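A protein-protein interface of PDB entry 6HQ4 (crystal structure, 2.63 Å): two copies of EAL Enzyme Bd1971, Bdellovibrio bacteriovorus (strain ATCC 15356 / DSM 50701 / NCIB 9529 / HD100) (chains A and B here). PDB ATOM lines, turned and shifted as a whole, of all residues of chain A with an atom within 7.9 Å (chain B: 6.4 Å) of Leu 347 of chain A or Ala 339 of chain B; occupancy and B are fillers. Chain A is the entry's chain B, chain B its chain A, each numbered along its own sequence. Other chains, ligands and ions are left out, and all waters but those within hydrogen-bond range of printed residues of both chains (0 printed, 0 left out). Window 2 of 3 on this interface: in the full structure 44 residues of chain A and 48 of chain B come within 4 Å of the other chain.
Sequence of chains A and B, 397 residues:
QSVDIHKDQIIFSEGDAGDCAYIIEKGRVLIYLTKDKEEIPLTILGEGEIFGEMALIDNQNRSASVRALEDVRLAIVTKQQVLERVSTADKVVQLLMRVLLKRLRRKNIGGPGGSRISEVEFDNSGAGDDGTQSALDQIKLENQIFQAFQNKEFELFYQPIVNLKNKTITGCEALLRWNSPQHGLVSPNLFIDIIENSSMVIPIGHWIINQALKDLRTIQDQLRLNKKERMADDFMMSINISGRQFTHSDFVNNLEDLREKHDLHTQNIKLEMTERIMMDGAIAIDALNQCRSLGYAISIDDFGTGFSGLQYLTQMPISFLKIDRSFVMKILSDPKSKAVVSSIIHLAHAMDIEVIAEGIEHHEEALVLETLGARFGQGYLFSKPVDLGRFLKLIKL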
ATOM      1  N   PHE A 303      15.668   4.961 -13.966  1.00  0.00           N
ATOM      2  CA  PHE A 303      15.637   3.522 -13.731  1.00  0.00           C
ATOM      3  C   PHE A 303      15.425   2.797 -15.062  1.00  0.00           C
ATOM      4  O   PHE A 303      14.611   3.222 -15.880  1.00  0.00           O
ATOM      5  CB  PHE A 303      14.522   3.168 -12.742  1.00  0.00           C
ATOM      6  CG  PHE A 303      14.400   1.696 -12.473  1.00  0.00           C
ATOM      7  CD1 PHE A 303      13.559   0.907 -13.243  1.00  0.00           C
ATOM      8  CD2 PHE A 303      15.132   1.095 -11.460  1.00  0.00           C
ATOM      9  CE1 PHE A 303      13.447  -0.452 -13.004  1.00  0.00           C
ATOM     10  CE2 PHE A 303      15.024  -0.265 -11.219  1.00  0.00           C
ATOM     11  CZ  PHE A 303      14.178  -1.039 -11.991  1.00  0.00           C
ATOM     12  N   GLY A 309      19.295  -2.306 -12.079  1.00  0.00           N
ATOM     13  CA  GLY A 309      18.734  -2.079 -10.770  1.00  0.00           C
ATOM     14  C   GLY A 309      18.282  -3.323 -10.075  1.00  0.00           C
ATOM     15  O   GLY A 309      18.395  -3.423  -8.867  1.00  0.00           O
ATOM     16  N   LEU A 310      17.805  -4.286 -10.845  1.00  0.00           N
ATOM     17  CA  LEU A 310      16.931  -5.317 -10.299  1.00  0.00           C
ATOM     18  C   LEU A 310      17.518  -6.025  -9.073  1.00  0.00           C
ATOM     19  O   LEU A 310      16.786  -6.344  -8.135  1.00  0.00           O
ATOM     20  CB  LEU A 310      16.542  -6.322 -11.386  1.00  0.00           C
ATOM     21  CG  LEU A 310      15.530  -5.925 -12.452  1.00  0.00           C
ATOM     22  CD1 LEU A 310      14.213  -5.543 -11.804  1.00  0.00           C
ATOM     23  CD2 LEU A 310      16.008  -4.817 -13.377  1.00  0.00           C
ATOM     24  N   LEU A 313      18.298  -3.233  -6.465  1.00  0.00           N
ATOM     25  CA  LEU A 313      17.011  -2.861  -5.929  1.00  0.00           C
ATOM     26  C   LEU A 313      16.645  -3.640  -4.657  1.00  0.00           C
ATOM     27  O   LEU A 313      15.969  -3.111  -3.773  1.00  0.00           O
ATOM     28  CB  LEU A 313      15.989  -3.072  -7.036  1.00  0.00           C
ATOM     29  CG  LEU A 313      14.681  -2.355  -6.937  1.00  0.00           C
ATOM     30  CD1 LEU A 313      14.069  -2.205  -8.321  1.00  0.00           C
ATOM     31  CD2 LEU A 313      13.810  -3.158  -6.015  1.00  0.00           C
ATOM     32  N   THR A 314      17.084  -4.891  -4.566  1.00  0.00           N
ATOM     33  CA  THR A 314      16.847  -5.703  -3.366  1.00  0.00           C
ATOM     34  C   THR A 314      17.773  -5.300  -2.213  1.00  0.00           C
ATOM     35  O   THR A 314      17.443  -5.531  -1.047  1.00  0.00           O
ATOM     36  CB  THR A 314      16.979  -7.220  -3.637  1.00  0.00           C
ATOM     37  OG1 THR A 314      18.029  -7.463  -4.583  1.00  0.00           O
ATOM     38  CG2 THR A 314      15.673  -7.795  -4.171  1.00  0.00           C
ATOM     39  N   LEU A 321      11.416   5.445  -7.464  1.00  0.00           N
ATOM     40  CA  LEU A 321      12.197   5.353  -8.691  1.00  0.00           C
ATOM     41  C   LEU A 321      11.492   6.138  -9.785  1.00  0.00           C
ATOM     42  O   LEU A 321      10.267   6.252  -9.783  1.00  0.00           O
ATOM     43  CB  LEU A 321      12.450   3.898  -9.101  1.00  0.00           C
ATOM     44  CG  LEU A 321      11.269   2.962  -9.359  1.00  0.00           C
ATOM     45  CD1 LEU A 321      10.759   3.075 -10.789  1.00  0.00           C
ATOM     46  CD2 LEU A 321      11.669   1.520  -9.076  1.00  0.00           C
ATOM     47  N   VAL A 340       6.845  -2.796 -20.748  1.00  0.00           N
ATOM     48  CA  VAL A 340       8.006  -2.552 -19.896  1.00  0.00           C
ATOM     49  C   VAL A 340       7.629  -1.647 -18.724  1.00  0.00           C
ATOM     50  O   VAL A 340       7.975  -1.929 -17.573  1.00  0.00           O
ATOM     51  CB  VAL A 340       9.165  -1.908 -20.689  1.00  0.00           C
ATOM     52  CG1 VAL A 340      10.269  -1.428 -19.752  1.00  0.00           C
ATOM     53  CG2 VAL A 340       9.727  -2.892 -21.701  1.00  0.00           C
ATOM     54  N   VAL A 341       6.911  -0.568 -19.026  1.00  0.00           N
ATOM     55  CA  VAL A 341       6.527   0.422 -18.021  1.00  0.00           C
ATOM     56  C   VAL A 341       5.526  -0.141 -17.029  1.00  0.00           C
ATOM     57  O   VAL A 341       5.661   0.077 -15.825  1.00  0.00           O
ATOM     58  CB  VAL A 341       5.988   1.710 -18.686  1.00  0.00           C
ATOM     59  CG1 VAL A 341       5.326   2.636 -17.667  1.00  0.00           C
ATOM     60  CG2 VAL A 341       7.134   2.421 -19.397  1.00  0.00           C
ATOM     61  N   SER A 342       4.521  -0.857 -17.525  1.00  0.00           N
ATOM     62  CA  SER A 342       3.565  -1.521 -16.642  1.00  0.00           C
ATOM     63  C   SER A 342       4.297  -2.403 -15.640  1.00  0.00           C
ATOM     64  O   SER A 342       3.980  -2.402 -14.449  1.00  0.00           O
ATOM     65  CB  SER A 342       2.580  -2.366 -17.442  1.00  0.00           C
ATOM     66  OG  SER A 342       1.617  -2.951 -16.583  1.00  0.00           O
ATOM     67  N   SER A 343       5.290  -3.135 -16.136  1.00  0.00           N
ATOM     68  CA  SER A 343       6.057  -4.079 -15.329  1.00  0.00           C
ATOM     69  C   SER A 343       6.900  -3.390 -14.250  1.00  0.00           C
ATOM     70  O   SER A 343       7.012  -3.902 -13.138  1.00  0.00           O
ATOM     71  CB  SER A 343       6.950  -4.932 -16.232  1.00  0.00           C
ATOM     72  OG  SER A 343       7.466  -6.046 -15.533  1.00  0.00           O
ATOM     73  N   ILE A 344       7.489  -2.241 -14.577  1.00  0.00           N
ATOM     74  CA  ILE A 344       8.264  -1.466 -13.598  1.00  0.00           C
ATOM     75  C   ILE A 344       7.366  -0.943 -12.473  1.00  0.00           C
ATOM     76  O   ILE A 344       7.742  -0.992 -11.300  1.00  0.00           O
ATOM     77  CB  ILE A 344       9.014  -0.285 -14.252  1.00  0.00           C
ATOM     78  CG1 ILE A 344      10.108  -0.802 -15.182  1.00  0.00           C
ATOM     79  CG2 ILE A 344       9.639   0.619 -13.193  1.00  0.00           C
ATOM     80  CD1 ILE A 344      10.666   0.240 -16.126  1.00  0.00           C
ATOM     81  N   ILE A 345       6.185  -0.446 -12.838  1.00  0.00           N
ATOM     82  CA  ILE A 345       5.229   0.072 -11.860  1.00  0.00           C
ATOM     83  C   ILE A 345       4.773  -1.032 -10.909  1.00  0.00           C
ATOM     84  O   ILE A 345       4.764  -0.846  -9.695  1.00  0.00           O
ATOM     85  CB  ILE A 345       4.001   0.713 -12.545  1.00  0.00           C
ATOM     86  CG1 ILE A 345       4.415   1.987 -13.288  1.00  0.00           C
ATOM     87  CG2 ILE A 345       2.918   1.043 -11.526  1.00  0.00           C
ATOM     88  CD1 ILE A 345       3.405   2.462 -14.314  1.00  0.00           C
ATOM     89  N   HIS A 346       4.412  -2.186 -11.464  1.00  0.00           N
ATOM     90  CA  HIS A 346       3.924  -3.298 -10.648  1.00  0.00           C
ATOM     91  C   HIS A 346       5.020  -3.827  -9.731  1.00  0.00           C
ATOM     92  O   HIS A 346       4.776  -4.095  -8.558  1.00  0.00           O
ATOM     93  CB  HIS A 346       3.345  -4.413 -11.525  1.00  0.00           C
ATOM     94  CG  HIS A 346       1.978  -4.102 -12.053  1.00  0.00           C
ATOM     95  ND1 HIS A 346       1.749  -3.123 -12.998  1.00  0.00           N
ATOM     96  CD2 HIS A 346       0.766  -4.625 -11.753  1.00  0.00           C
ATOM     97  CE1 HIS A 346       0.457  -3.063 -13.263  1.00  0.00           C
ATOM     98  NE2 HIS A 346      -0.162  -3.966 -12.522  1.00  0.00           N
ATOM     99  N   LEU A 347       6.230  -3.955 -10.267  1.00  0.00           N
ATOM    100  CA  LEU A 347       7.378  -4.374  -9.471  1.00  0.00           C
ATOM    101  C   LEU A 347       7.648  -3.379  -8.340  1.00  0.00           C
ATOM    102  O   LEU A 347       7.822  -3.778  -7.186  1.00  0.00           O
ATOM    103  CB  LEU A 347       8.618  -4.522 -10.354  1.00  0.00           C
ATOM    104  CG  LEU A 347       9.901  -4.934  -9.630  1.00  0.00           C
ATOM    105  CD1 LEU A 347       9.700  -6.225  -8.848  1.00  0.00           C
ATOM    106  CD2 LEU A 347      11.060  -5.064 -10.604  1.00  0.00           C
ATOM    107  N   ALA A 348       7.671  -2.090  -8.671  1.00  0.00           N
ATOM    108  CA  ALA A 348       7.853  -1.041  -7.667  1.00  0.00           C
ATOM    109  C   ALA A 348       6.849  -1.181  -6.521  1.00  0.00           C
ATOM    110  O   ALA A 348       7.240  -1.162  -5.354  1.00  0.00           O
ATOM    111  CB  ALA A 348       7.739   0.335  -8.305  1.00  0.00           C
ATOM    112  N   HIS A 349       5.567  -1.340  -6.857  1.00  0.00           N
ATOM    113  CA  HIS A 349       4.523  -1.514  -5.838  1.00  0.00           C
ATOM    114  C   HIS A 349       4.803  -2.717  -4.948  1.00  0.00           C
ATOM    115  O   HIS A 349       4.597  -2.659  -3.739  1.00  0.00           O
ATOM    116  CB  HIS A 349       3.135  -1.719  -6.452  1.00  0.00           C
ATOM    117  CG  HIS A 349       2.589  -0.528  -7.175  1.00  0.00           C
ATOM    118  ND1 HIS A 349       1.593  -0.639  -8.120  1.00  0.00           N
ATOM    119  CD2 HIS A 349       2.883   0.790  -7.087  1.00  0.00           C
ATOM    120  CE1 HIS A 349       1.296   0.563  -8.585  1.00  0.00           C
ATOM    121  NE2 HIS A 349       2.064   1.447  -7.975  1.00  0.00           N
ATOM    122  N   ALA A 350       5.272  -3.803  -5.553  1.00  0.00           N
ATOM    123  CA  ALA A 350       5.531  -5.052  -4.833  1.00  0.00           C
ATOM    124  C   ALA A 350       6.601  -4.942  -3.740  1.00  0.00           C
ATOM    125  O   ALA A 350       6.758  -5.864  -2.940  1.00  0.00           O
ATOM    126  CB  ALA A 350       5.904  -6.151  -5.815  1.00  0.00           C
ATOM    127  N   MET A 351       7.345  -3.837  -3.718  1.00  0.00           N
ATOM    128  CA  MET A 351       8.363  -3.608  -2.698  1.00  0.00           C
ATOM    129  C   MET A 351       8.177  -2.259  -2.011  1.00  0.00           C
ATOM    130  O   MET A 351       9.144  -1.663  -1.533  1.00  0.00           O
ATOM    131  CB  MET A 351       9.743  -3.676  -3.339  1.00  0.00           C
ATOM    132  CG  MET A 351       9.865  -4.805  -4.339  1.00  0.00           C
ATOM    133  SD  MET A 351      11.493  -4.854  -5.095  1.00  0.00           S
ATOM    134  CE  MET A 351      11.055  -4.017  -6.619  1.00  0.00           C
ATOM    135  N   ASP A 352       6.930  -1.795  -1.949  1.00  0.00           N
ATOM    136  CA  ASP A 352       6.593  -0.506  -1.347  1.00  0.00           C
ATOM    137  C   ASP A 352       7.518   0.615  -1.845  1.00  0.00           C
ATOM    138  O   ASP A 352       8.063   1.386  -1.056  1.00  0.00           O
ATOM    139  CB  ASP A 352       6.615  -0.625   0.188  1.00  0.00           C
ATOM    140  CG  ASP A 352       5.587  -1.628   0.723  1.00  0.00           C
ATOM    141  OD1 ASP A 352       4.481  -1.764   0.149  1.00  0.00           O
ATOM    142  OD2 ASP A 352       5.896  -2.293   1.739  1.00  0.00           O
ATOM    143  N   ILE A 353       7.700   0.676  -3.163  1.00  0.00           N
ATOM    144  CA  ILE A 353       8.377   1.790  -3.817  1.00  0.00           C
ATOM    145  C   ILE A 353       7.319   2.503  -4.641  1.00  0.00           C
ATOM    146  O   ILE A 353       6.464   1.857  -5.241  1.00  0.00           O
ATOM    147  CB  ILE A 353       9.535   1.321  -4.731  1.00  0.00           C
ATOM    148  CG1 ILE A 353      10.618   0.632  -3.902  1.00  0.00           C
ATOM    149  CG2 ILE A 353      10.148   2.499  -5.484  1.00  0.00           C
ATOM    150  CD1 ILE A 353      11.686  -0.059  -4.727  1.00  0.00           C
ATOM    151  N   VAL A 355       6.323   5.449  -7.720  1.00  0.00           N
ATOM    152  CA  VAL A 355       6.825   5.768  -9.052  1.00  0.00           C
ATOM    153  C   VAL A 355       6.537   7.215  -9.452  1.00  0.00           C
ATOM    154  O   VAL A 355       5.454   7.740  -9.193  1.00  0.00           O
ATOM    155  CB  VAL A 355       6.197   4.833 -10.105  1.00  0.00           C
ATOM    156  CG1 VAL A 355       6.712   5.158 -11.497  1.00  0.00           C
ATOM    157  CG2 VAL A 355       6.485   3.377  -9.761  1.00  0.00           C
ATOM    158  N   ILE B 331      15.513 -16.603  -3.511  1.00  0.00           N
ATOM    159  CA  ILE B 331      14.081 -16.611  -3.803  1.00  0.00           C
ATOM    160  C   ILE B 331      13.239 -17.015  -2.589  1.00  0.00           C
ATOM    161  O   ILE B 331      12.202 -16.411  -2.323  1.00  0.00           O
ATOM    162  CB  ILE B 331      13.768 -17.514  -5.025  1.00  0.00           C
ATOM    163  CG1 ILE B 331      12.362 -17.226  -5.556  1.00  0.00           C
ATOM    164  CG2 ILE B 331      13.963 -18.993  -4.698  1.00  0.00           C
ATOM    165  CD1 ILE B 331      12.029 -17.952  -6.841  1.00  0.00           C
ATOM    166  N   ASP B 334      14.502 -14.366   0.838  1.00  0.00           N
ATOM    167  CA  ASP B 334      14.217 -12.948   0.613  1.00  0.00           C
ATOM    168  C   ASP B 334      12.954 -12.823  -0.252  1.00  0.00           C
ATOM    169  O   ASP B 334      12.984 -13.136  -1.441  1.00  0.00           O
ATOM    170  CB  ASP B 334      15.422 -12.294  -0.073  1.00  0.00           C
ATOM    171  CG  ASP B 334      15.328 -10.779  -0.134  1.00  0.00           C
ATOM    172  OD1 ASP B 334      14.351 -10.204   0.390  1.00  0.00           O
ATOM    173  OD2 ASP B 334      16.245 -10.160  -0.712  1.00  0.00           O
ATOM    174  N   PRO B 335      11.835 -12.367   0.343  1.00  0.00           N
ATOM    175  CA  PRO B 335      10.552 -12.415  -0.367  1.00  0.00           C
ATOM    176  C   PRO B 335      10.386 -11.360  -1.467  1.00  0.00           C
ATOM    177  O   PRO B 335       9.461 -11.472  -2.274  1.00  0.00           O
ATOM    178  CB  PRO B 335       9.534 -12.178   0.749  1.00  0.00           C
ATOM    179  CG  PRO B 335      10.256 -11.317   1.726  1.00  0.00           C
ATOM    180  CD  PRO B 335      11.703 -11.725   1.667  1.00  0.00           C
ATOM    181  N   LYS B 336      11.249 -10.346  -1.486  1.00  0.00           N
ATOM    182  CA  LYS B 336      11.204  -9.327  -2.535  1.00  0.00           C
ATOM    183  C   LYS B 336      12.204  -9.606  -3.657  1.00  0.00           C
ATOM    184  O   LYS B 336      12.071  -9.063  -4.750  1.00  0.00           O
ATOM    185  CB  LYS B 336      11.391  -7.920  -1.950  1.00  0.00           C
ATOM    186  CG  LYS B 336      12.785  -7.599  -1.444  1.00  0.00           C
ATOM    187  CD  LYS B 336      12.806  -6.307  -0.647  1.00  0.00           C
ATOM    188  CE  LYS B 336      14.241  -5.916  -0.358  1.00  0.00           C
ATOM    189  NZ  LYS B 336      14.326  -4.711   0.503  1.00  0.00           N
ATOM    190  N   SER B 337      13.192 -10.461  -3.392  1.00  0.00           N
ATOM    191  CA  SER B 337      13.997 -11.058  -4.463  1.00  0.00           C
ATOM    192  C   SER B 337      13.134 -12.005  -5.306  1.00  0.00           C
ATOM    193  O   SER B 337      13.374 -12.169  -6.499  1.00  0.00           O
ATOM    194  CB  SER B 337      15.210 -11.809  -3.899  1.00  0.00           C
ATOM    195  OG  SER B 337      16.224 -10.913  -3.479  1.00  0.00           O
ATOM    196  N   LYS B 338      12.137 -12.626  -4.678  1.00  0.00           N
ATOM    197  CA  LYS B 338      11.139 -13.420  -5.397  1.00  0.00           C
ATOM    198  C   LYS B 338      10.327 -12.539  -6.346  1.00  0.00           C
ATOM    199  O   LYS B 338      10.038 -12.934  -7.480  1.00  0.00           O
ATOM    200  CB  LYS B 338      10.205 -14.130  -4.408  1.00  0.00           C
ATOM    201  CG  LYS B 338       9.121 -14.975  -5.071  1.00  0.00           C
ATOM    202  CD  LYS B 338       8.566 -16.087  -4.182  1.00  0.00           C
ATOM    203  CE  LYS B 338       7.746 -15.581  -3.004  1.00  0.00           C
ATOM    204  NZ  LYS B 338       7.062 -16.699  -2.290  1.00  0.00           N
ATOM    205  N   ALA B 339       9.961 -11.349  -5.869  1.00  0.00           N
ATOM    206  CA  ALA B 339       9.182 -10.388  -6.654  1.00  0.00           C
ATOM    207  C   ALA B 339       9.939  -9.911  -7.889  1.00  0.00           C
ATOM    208  O   ALA B 339       9.352  -9.742  -8.956  1.00  0.00           O
ATOM    209  CB  ALA B 339       8.784  -9.200  -5.790  1.00  0.00           C
ATOM    210  N   VAL B 340      11.238  -9.689  -7.738  1.00  0.00           N
ATOM    211  CA  VAL B 340      12.079  -9.314  -8.865  1.00  0.00           C
ATOM    212  C   VAL B 340      12.032 -10.396  -9.947  1.00  0.00           C
ATOM    213  O   VAL B 340      11.871 -10.087 -11.127  1.00  0.00           O
ATOM    214  CB  VAL B 340      13.538  -9.092  -8.420  1.00  0.00           C
ATOM    215  CG1 VAL B 340      14.463  -8.963  -9.620  1.00  0.00           C
ATOM    216  CG2 VAL B 340      13.644  -7.849  -7.540  1.00  0.00           C
ATOM    217  N   VAL B 341      12.163 -11.655  -9.531  1.00  0.00           N
ATOM    218  CA  VAL B 341      12.207 -12.784 -10.454  1.00  0.00           C
ATOM    219  C   VAL B 341      10.863 -13.015 -11.139  1.00  0.00           C
ATOM    220  O   VAL B 341      10.813 -13.230 -12.347  1.00  0.00           O
ATOM    221  CB  VAL B 341      12.687 -14.070  -9.742  1.00  0.00           C
ATOM    222  CG1 VAL B 341      12.465 -15.309 -10.609  1.00  0.00           C
ATOM    223  CG2 VAL B 341      14.160 -13.932  -9.371  1.00  0.00           C
ATOM    224  N   SER B 342       9.779 -12.960 -10.375  1.00  0.00           N
ATOM    225  CA  SER B 342       8.443 -13.043 -10.961  1.00  0.00           C
ATOM    226  C   SER B 342       8.274 -12.008 -12.069  1.00  0.00           C
ATOM    227  O   SER B 342       7.751 -12.313 -13.144  1.00  0.00           O
ATOM    228  CB  SER B 342       7.372 -12.822  -9.897  1.00  0.00           C
ATOM    229  OG  SER B 342       6.081 -12.971 -10.460  1.00  0.00           O
ATOM    230  N   SER B 343       8.740 -10.790 -11.798  1.00  0.00           N
ATOM    231  CA  SER B 343       8.596  -9.669 -12.719  1.00  0.00           C
ATOM    232  C   SER B 343       9.401  -9.858 -14.005  1.00  0.00           C
ATOM    233  O   SER B 343       8.935  -9.493 -15.083  1.00  0.00           O
ATOM    234  CB  SER B 343       9.012  -8.366 -12.026  1.00  0.00           C
ATOM    235  OG  SER B 343       8.618  -7.235 -12.776  1.00  0.00           O
ATOM    236  N   ILE B 344      10.606 -10.416 -13.891  1.00  0.00           N
ATOM    237  CA  ILE B 344      11.435 -10.701 -15.065  1.00  0.00           C
ATOM    238  C   ILE B 344      10.780 -11.759 -15.962  1.00  0.00           C
ATOM    239  O   ILE B 344      10.779 -11.628 -17.185  1.00  0.00           O
ATOM    240  CB  ILE B 344      12.853 -11.171 -14.668  1.00  0.00           C
ATOM    241  CG1 ILE B 344      13.631 -10.024 -14.018  1.00  0.00           C
ATOM    242  CG2 ILE B 344      13.618 -11.664 -15.889  1.00  0.00           C
ATOM    243  CD1 ILE B 344      14.890 -10.458 -13.295  1.00  0.00           C
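The side-chain carboxylate (OD2) of Asp 334 of chain B lies within hydrogen-bond range of the side-chain hydroxyl (OG) of Ser 337 of chain B, at 2.9 Å.
Printed residues of chain B within 4 Å of Leu 310 of chain A: Val 340.
Of chain B, only Ala 339, Val 340 and Ser 343 come within 4 Å of Leu 347 of chain A.
Of the printed residues of chain A, Ser 337 of chain B touches Thr 314 (3.2 Å).
Ala 339 of chain B touches just one residue of chain A: Leu 347.
The nearest residue of chain A that does not touch Ala 339 of chain B is Ala 350 of chain A (4.2 Å).
The nearest printed residue of chain A that does not touch Ser 337 of chain B is Met 351 of chain A (6.1 Å).
Hydrophobic or aromatic side chains of chain A within 4 Å of the printed part of chain B: Leu 310 and Leu 347.
Printed residues of chain B that touch a printed residue of chain A: Lys 336, Ser 337, Ala 339, Val 340 and Ser 343.
Among the printed residues, 8 pairs touch across the chains.
Ser 343 of chain B touches its own counterpart, Ser 343 of chain A.
Among the printed residues, merely in contact across the chains: Leu 310 of chain A with Val 340 of chain B (3.5 Å), Thr 314 of chain A with Lys 336 of chain B (3.3 Å), Thr 314 of chain A with Ser 337 of chain B (3.2 Å), Thr 314 of chain A with Val 340 of chain B (3.9 Å), Leu 347 of chain A with Ala 339 of chain B (3.5 Å), Leu 347 of chain A with Val 340 of chain B (3.9 Å) and Leu 347 of chain A with Ser 343 of chain B (3.6 Å).
OG of Ser 343 of chain B sits at hydrogen-bond distance from OG of Ser 343 of chain A, at 3.2 Å.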
